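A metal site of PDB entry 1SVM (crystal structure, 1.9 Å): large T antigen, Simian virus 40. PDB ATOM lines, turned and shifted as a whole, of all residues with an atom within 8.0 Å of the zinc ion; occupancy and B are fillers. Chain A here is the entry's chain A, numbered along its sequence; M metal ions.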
ATOM      1  N   GLU A  44      22.256  28.433   5.522  1.00  0.00           N
ATOM      2  CA  GLU A  44      21.951  27.209   6.279  1.00  0.00           C
ATOM      3  C   GLU A  44      23.226  26.468   6.665  1.00  0.00           C
ATOM      4  O   GLU A  44      23.218  25.656   7.587  1.00  0.00           O
ATOM      5  CB  GLU A  44      21.063  26.242   5.469  1.00  0.00           C
ATOM      6  CG  GLU A  44      19.684  26.767   5.107  1.00  0.00           C
ATOM      7  CD  GLU A  44      18.796  25.681   4.514  1.00  0.00           C
ATOM      8  OE1 GLU A  44      19.335  24.766   3.854  1.00  0.00           O
ATOM      9  OE2 GLU A  44      17.561  25.746   4.685  1.00  0.00           O
ATOM     10  N   PHE A  45      24.327  26.754   5.958  1.00  0.00           N
ATOM     11  CA  PHE A  45      25.589  26.083   6.239  1.00  0.00           C
ATOM     12  C   PHE A  45      26.385  26.716   7.380  1.00  0.00           C
ATOM     13  O   PHE A  45      27.387  26.145   7.812  1.00  0.00           O
ATOM     14  CB  PHE A  45      26.494  26.071   4.989  1.00  0.00           C
ATOM     15  CG  PHE A  45      25.899  25.370   3.789  1.00  0.00           C
ATOM     16  CD1 PHE A  45      25.076  24.259   3.950  1.00  0.00           C
ATOM     17  CD2 PHE A  45      26.203  25.808   2.498  1.00  0.00           C
ATOM     18  CE1 PHE A  45      24.556  23.587   2.820  1.00  0.00           C
ATOM     19  CE2 PHE A  45      25.692  25.156   1.373  1.00  0.00           C
ATOM     20  CZ  PHE A  45      24.868  24.035   1.534  1.00  0.00           C
ATOM     21  N   TYR A  47      25.671  26.978  10.441  1.00  0.00           N
ATOM     22  CA  TYR A  47      25.541  26.233  11.687  1.00  0.00           C
ATOM     23  C   TYR A  47      26.305  24.905  11.622  1.00  0.00           C
ATOM     24  O   TYR A  47      26.488  24.329  10.546  1.00  0.00           O
ATOM     25  CB  TYR A  47      24.055  25.957  11.957  1.00  0.00           C
ATOM     26  CG  TYR A  47      23.194  27.196  11.892  1.00  0.00           C
ATOM     27  CD1 TYR A  47      23.214  28.155  12.907  1.00  0.00           C
ATOM     28  CD2 TYR A  47      22.365  27.425  10.785  1.00  0.00           C
ATOM     29  CE1 TYR A  47      22.442  29.312  12.829  1.00  0.00           C
ATOM     30  CE2 TYR A  47      21.590  28.582  10.694  1.00  0.00           C
ATOM     31  CZ  TYR A  47      21.626  29.520  11.720  1.00  0.00           C
ATOM     32  OH  TYR A  47      20.864  30.657  11.626  1.00  0.00           O
ATOM     33  N   SER A  48      26.741  24.431  12.793  1.00  0.00           N
ATOM     34  CA  SER A  48      27.493  23.175  12.897  1.00  0.00           C
ATOM     35  C   SER A  48      26.908  22.057  12.035  1.00  0.00           C
ATOM     36  O   SER A  48      25.706  21.788  12.083  1.00  0.00           O
ATOM     37  CB  SER A  48      27.509  22.717  14.357  1.00  0.00           C
ATOM     38  OG  SER A  48      27.821  21.336  14.456  1.00  0.00           O
ATOM     39  N   PHE A  49      27.763  21.380  11.261  1.00  0.00           N
ATOM     40  CA  PHE A  49      27.284  20.278  10.420  1.00  0.00           C
ATOM     41  C   PHE A  49      27.165  18.978  11.215  1.00  0.00           C
ATOM     42  O   PHE A  49      26.451  18.059  10.823  1.00  0.00           O
ATOM     43  CB  PHE A  49      28.197  20.086   9.205  1.00  0.00           C
ATOM     44  CG  PHE A  49      29.616  19.740   9.552  1.00  0.00           C
ATOM     45  CD1 PHE A  49      29.981  18.419   9.813  1.00  0.00           C
ATOM     46  CD2 PHE A  49      30.587  20.737   9.619  1.00  0.00           C
ATOM     47  CE1 PHE A  49      31.303  18.106  10.145  1.00  0.00           C
ATOM     48  CE2 PHE A  49      31.910  20.425   9.950  1.00  0.00           C
ATOM     49  CZ  PHE A  49      32.274  19.104  10.212  1.00  0.00           C
ATOM     50  N   GLU A  50      27.863  18.914  12.350  1.00  0.00           N
ATOM     51  CA  GLU A  50      27.827  17.733  13.207  1.00  0.00           C
ATOM     52  C   GLU A  50      26.546  17.644  14.018  1.00  0.00           C
ATOM     53  O   GLU A  50      26.183  16.570  14.519  1.00  0.00           O
ATOM     54  CB  GLU A  50      29.044  17.719  14.126  1.00  0.00           C
ATOM     55  CG  GLU A  50      30.351  17.487  13.389  1.00  0.00           C
ATOM     56  CD  GLU A  50      31.574  17.802  14.220  1.00  0.00           C
ATOM     57  OE1 GLU A  50      31.734  18.981  14.618  1.00  0.00           O
ATOM     58  OE2 GLU A  50      32.385  16.886  14.470  1.00  0.00           O
ATOM     59  N   MET A  51      25.858  18.770  14.161  1.00  0.00           N
ATOM     60  CA  MET A  51      24.611  18.809  14.906  1.00  0.00           C
ATOM     61  C   MET A  51      23.528  19.389  14.008  1.00  0.00           C
ATOM     62  O   MET A  51      22.738  20.230  14.427  1.00  0.00           O
ATOM     63  CB  MET A  51      24.757  19.686  16.147  1.00  0.00           C
ATOM     64  CG  MET A  51      25.805  19.188  17.141  1.00  0.00           C
ATOM     65  SD  MET A  51      25.851  20.220  18.621  1.00  0.00           S
ATOM     66  CE  MET A  51      26.892  21.580  18.057  1.00  0.00           C
ATOM     67  N   CYS A  52      23.504  18.918  12.761  1.00  0.00           N
ATOM     68  CA  CYS A  52      22.533  19.393  11.794  1.00  0.00           C
ATOM     69  C   CYS A  52      21.425  18.398  11.497  1.00  0.00           C
ATOM     70  O   CYS A  52      21.679  17.304  10.993  1.00  0.00           O
ATOM     71  CB  CYS A  52      23.232  19.778  10.495  1.00  0.00           C
ATOM     72  SG  CYS A  52      22.089  20.347   9.226  1.00  0.00           S
ATOM     73  N   LEU A  53      20.198  18.784  11.817  1.00  0.00           N
ATOM     74  CA  LEU A  53      19.048  17.931  11.572  1.00  0.00           C
ATOM     75  C   LEU A  53      18.806  17.716  10.083  1.00  0.00           C
ATOM     76  O   LEU A  53      18.487  16.612   9.641  1.00  0.00           O
ATOM     77  CB  LEU A  53      17.790  18.540  12.211  1.00  0.00           C
ATOM     78  CG  LEU A  53      16.486  17.763  12.007  1.00  0.00           C
ATOM     79  CD1 LEU A  53      16.666  16.309  12.440  1.00  0.00           C
ATOM     80  CD2 LEU A  53      15.375  18.429  12.808  1.00  0.00           C
ATOM     81  N   LYS A  54      18.961  18.784   9.295  1.00  0.00           N
ATOM     82  CA  LYS A  54      18.755  18.698   7.849  1.00  0.00           C
ATOM     83  C   LYS A  54      19.687  17.660   7.254  1.00  0.00           C
ATOM     84  O   LYS A  54      19.303  16.915   6.355  1.00  0.00           O
ATOM     85  CB  LYS A  54      18.983  20.055   7.181  1.00  0.00           C
ATOM     86  CG  LYS A  54      17.964  21.124   7.542  1.00  0.00           C
ATOM     87  CD  LYS A  54      18.239  22.429   6.799  1.00  0.00           C
ATOM     88  CE  LYS A  54      17.281  23.537   7.233  1.00  0.00           C
ATOM     89  NZ  LYS A  54      15.865  23.183   6.945  1.00  0.00           N
ATOM     90  N   CYS A  55      20.919  17.612   7.757  1.00  0.00           N
ATOM     91  CA  CYS A  55      21.886  16.644   7.241  1.00  0.00           C
ATOM     92  C   CYS A  55      21.539  15.208   7.645  1.00  0.00           C
ATOM     93  O   CYS A  55      21.678  14.286   6.848  1.00  0.00           O
ATOM     94  CB  CYS A  55      23.298  16.999   7.704  1.00  0.00           C
ATOM     95  SG  CYS A  55      24.136  18.262   6.692  1.00  0.00           S
ATOM     96  N   ILE A  56      21.074  15.035   8.885  1.00  0.00           N
ATOM     97  CA  ILE A  56      20.723  13.701   9.355  1.00  0.00           C
ATOM     98  C   ILE A  56      19.470  13.137   8.690  1.00  0.00           C
ATOM     99  O   ILE A  56      19.409  11.936   8.416  1.00  0.00           O
ATOM    100  CB  ILE A  56      20.525  13.671  10.890  1.00  0.00           C
ATOM    101  CG1 ILE A  56      21.828  14.042  11.580  1.00  0.00           C
ATOM    102  CG2 ILE A  56      20.099  12.279  11.326  1.00  0.00           C
ATOM    103  CD1 ILE A  56      21.824  13.756  13.058  1.00  0.00           C
ATOM    104  N   LYS A  58      18.582  13.743   5.779  1.00  0.00           N
ATOM    105  CA  LYS A  58      18.877  13.620   4.345  1.00  0.00           C
ATOM    106  C   LYS A  58      17.671  14.044   3.503  1.00  0.00           C
ATOM    107  O   LYS A  58      17.209  13.292   2.650  1.00  0.00           O
ATOM    108  CB  LYS A  58      19.262  12.172   3.995  1.00  0.00           C
ATOM    109  CG  LYS A  58      20.526  11.675   4.687  1.00  0.00           C
ATOM    110  CD  LYS A  58      21.745  12.510   4.323  1.00  0.00           C
ATOM    111  CE  LYS A  58      22.975  12.084   5.110  1.00  0.00           C
ATOM    112  NZ  LYS A  58      24.102  13.055   4.969  1.00  0.00           N
ATOM    113  N   GLN A  60      17.371  17.240   1.646  1.00  0.00           N
ATOM    114  CA  GLN A  60      17.703  17.978   0.435  1.00  0.00           C
ATOM    115  C   GLN A  60      19.166  17.794   0.033  1.00  0.00           C
ATOM    116  O   GLN A  60      20.060  18.319   0.683  1.00  0.00           O
ATOM    117  CB  GLN A  60      17.443  19.470   0.650  1.00  0.00           C
ATOM    118  CG  GLN A  60      15.978  19.823   0.914  1.00  0.00           C
ATOM    119  CD  GLN A  60      15.094  19.572  -0.295  1.00  0.00           C
ATOM    120  OE1 GLN A  60      15.549  19.637  -1.431  1.00  0.00           O
ATOM    121  NE2 GLN A  60      13.821  19.298  -0.043  1.00  0.00           N
ATOM    122  N   HIS A  63      21.588  20.402   0.039  1.00  0.00           N
ATOM    123  CA  HIS A  63      22.037  20.839   1.344  1.00  0.00           C
ATOM    124  C   HIS A  63      23.047  19.859   1.948  1.00  0.00           C
ATOM    125  O   HIS A  63      24.209  20.200   2.134  1.00  0.00           O
ATOM    126  CB  HIS A  63      20.875  20.967   2.332  1.00  0.00           C
ATOM    127  CG  HIS A  63      21.333  21.214   3.744  1.00  0.00           C
ATOM    128  ND1 HIS A  63      21.649  22.468   4.215  1.00  0.00           N
ATOM    129  CD2 HIS A  63      21.630  20.352   4.744  1.00  0.00           C
ATOM    130  CE1 HIS A  63      22.119  22.363   5.444  1.00  0.00           C
ATOM    131  NE2 HIS A  63      22.112  21.096   5.788  1.00  0.00           N
ATOM    132  N   TYR A  64      22.580  18.636   2.234  1.00  0.00           N
ATOM    133  CA  TYR A  64      23.430  17.652   2.902  1.00  0.00           C
ATOM    134  C   TYR A  64      24.685  17.183   2.199  1.00  0.00           C
ATOM    135  O   TYR A  64      25.618  16.726   2.856  1.00  0.00           O
ATOM    136  CB  TYR A  64      22.584  16.445   3.373  1.00  0.00           C
ATOM    137  CG  TYR A  64      22.032  15.524   2.301  1.00  0.00           C
ATOM    138  CD1 TYR A  64      22.862  14.639   1.612  1.00  0.00           C
ATOM    139  CD2 TYR A  64      20.669  15.518   2.000  1.00  0.00           C
ATOM    140  CE1 TYR A  64      22.352  13.757   0.661  1.00  0.00           C
ATOM    141  CE2 TYR A  64      20.145  14.647   1.052  1.00  0.00           C
ATOM    142  CZ  TYR A  64      20.987  13.762   0.383  1.00  0.00           C
ATOM    143  OH  TYR A  64      20.481  12.900  -0.554  1.00  0.00           O
ATOM    144  N   LYS A  65      24.739  17.319   0.876  1.00  0.00           N
ATOM    145  CA  LYS A  65      25.944  16.911   0.162  1.00  0.00           C
ATOM    146  C   LYS A  65      27.001  18.006   0.210  1.00  0.00           C
ATOM    147  O   LYS A  65      28.155  17.763  -0.138  1.00  0.00           O
ATOM    148  CB  LYS A  65      25.604  16.570  -1.290  1.00  0.00           C
ATOM    149  CG  LYS A  65      24.989  15.188  -1.486  1.00  0.00           C
ATOM    150  CD  LYS A  65      24.267  15.041  -2.832  1.00  0.00           C
ATOM    151  CE  LYS A  65      25.178  15.339  -4.004  1.00  0.00           C
ATOM    152  NZ  LYS A  65      24.440  15.273  -5.304  1.00  0.00           N
ATOM    153  N   TYR A  66      26.627  19.193   0.682  1.00  0.00           N
ATOM    154  CA  TYR A  66      27.569  20.312   0.727  1.00  0.00           C
ATOM    155  C   TYR A  66      27.851  20.985   2.061  1.00  0.00           C
ATOM    156  O   TYR A  66      28.834  21.732   2.191  1.00  0.00           O
ATOM    157  CB  TYR A  66      27.115  21.390  -0.261  1.00  0.00           C
ATOM    158  CG  TYR A  66      26.951  20.882  -1.679  1.00  0.00           C
ATOM    159  CD1 TYR A  66      25.754  20.290  -2.081  1.00  0.00           C
ATOM    160  CD2 TYR A  66      27.999  20.958  -2.591  1.00  0.00           C
ATOM    161  CE1 TYR A  66      25.608  19.773  -3.380  1.00  0.00           C
ATOM    162  CE2 TYR A  66      27.870  20.441  -3.880  1.00  0.00           C
ATOM    163  CZ  TYR A  66      26.676  19.848  -4.268  1.00  0.00           C
ATOM    164  OH  TYR A  66      26.544  19.331  -5.534  1.00  0.00           O
ATOM    165  N   HIS A  67      27.005  20.753   3.059  1.00  0.00           N
ATOM    166  CA  HIS A  67      27.169  21.409   4.354  1.00  0.00           C
ATOM    167  C   HIS A  67      28.564  21.336   4.974  1.00  0.00           C
ATOM    168  O   HIS A  67      29.161  22.359   5.311  1.00  0.00           O
ATOM    169  CB  HIS A  67      26.123  20.863   5.353  1.00  0.00           C
ATOM    170  CG  HIS A  67      25.979  21.680   6.600  1.00  0.00           C
ATOM    171  ND1 HIS A  67      25.003  21.432   7.540  1.00  0.00           N
ATOM    172  CD2 HIS A  67      26.682  22.750   7.052  1.00  0.00           C
ATOM    173  CE1 HIS A  67      25.114  22.317   8.520  1.00  0.00           C
ATOM    174  NE2 HIS A  67      26.119  23.121   8.247  1.00  0.00           N
ATOM    175  N   GLU A  68      29.086  20.129   5.142  1.00  0.00           N
ATOM    176  CA  GLU A  68      30.391  19.959   5.767  1.00  0.00           C
ATOM    177  C   GLU A  68      31.497  20.715   5.037  1.00  0.00           C
ATOM    178  O   GLU A  68      32.280  21.434   5.646  1.00  0.00           O
ATOM    179  CB  GLU A  68      30.746  18.467   5.850  1.00  0.00           C
ATOM    180  CG  GLU A  68      32.127  18.194   6.408  1.00  0.00           C
ATOM    181  CD  GLU A  68      32.325  16.730   6.757  1.00  0.00           C
ATOM    182  OE1 GLU A  68      31.872  15.858   5.996  1.00  0.00           O
ATOM    183  OE2 GLU A  68      32.952  16.457   7.807  1.00  0.00           O
HETATM  184 ZN    ZN M   1      23.429  20.244   7.367  1.00  0.00          ZN
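NE2 of His 67 sits at hydrogen-bond distance from O of Phe 45 (3.3 Å).
The backbone carbonyl oxygen (O) of Tyr 47 sits at hydrogen-bond distance from a ring nitrogen (NE2) of His 67 (2.6 Å).
O of Cys 55 sits close to NZ of Lys 58 (3.3 Å).
ND1 of His 63 sits at hydrogen-bond distance from OE1 of Glu 44 (3.3 Å).
SG of Cys 52 sits close to N of Lys 54, at 3.5 Å.
Four residues have an atom within 4 Å of the zinc ion: Cys 52, Cys 55, His 63 and His 67.
The nearest printed residue that does not touch the zinc ion is Lys 54 (4.5 Å).
The zinc ion is bound by a ring nitrogen (ND1) of His 67, the side-chain sulfur of Cys 55, a ring nitrogen (NE2) of His 63 and the side-chain sulfur of Cys 52.
The zinc ion has four donor atoms within binding distance.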
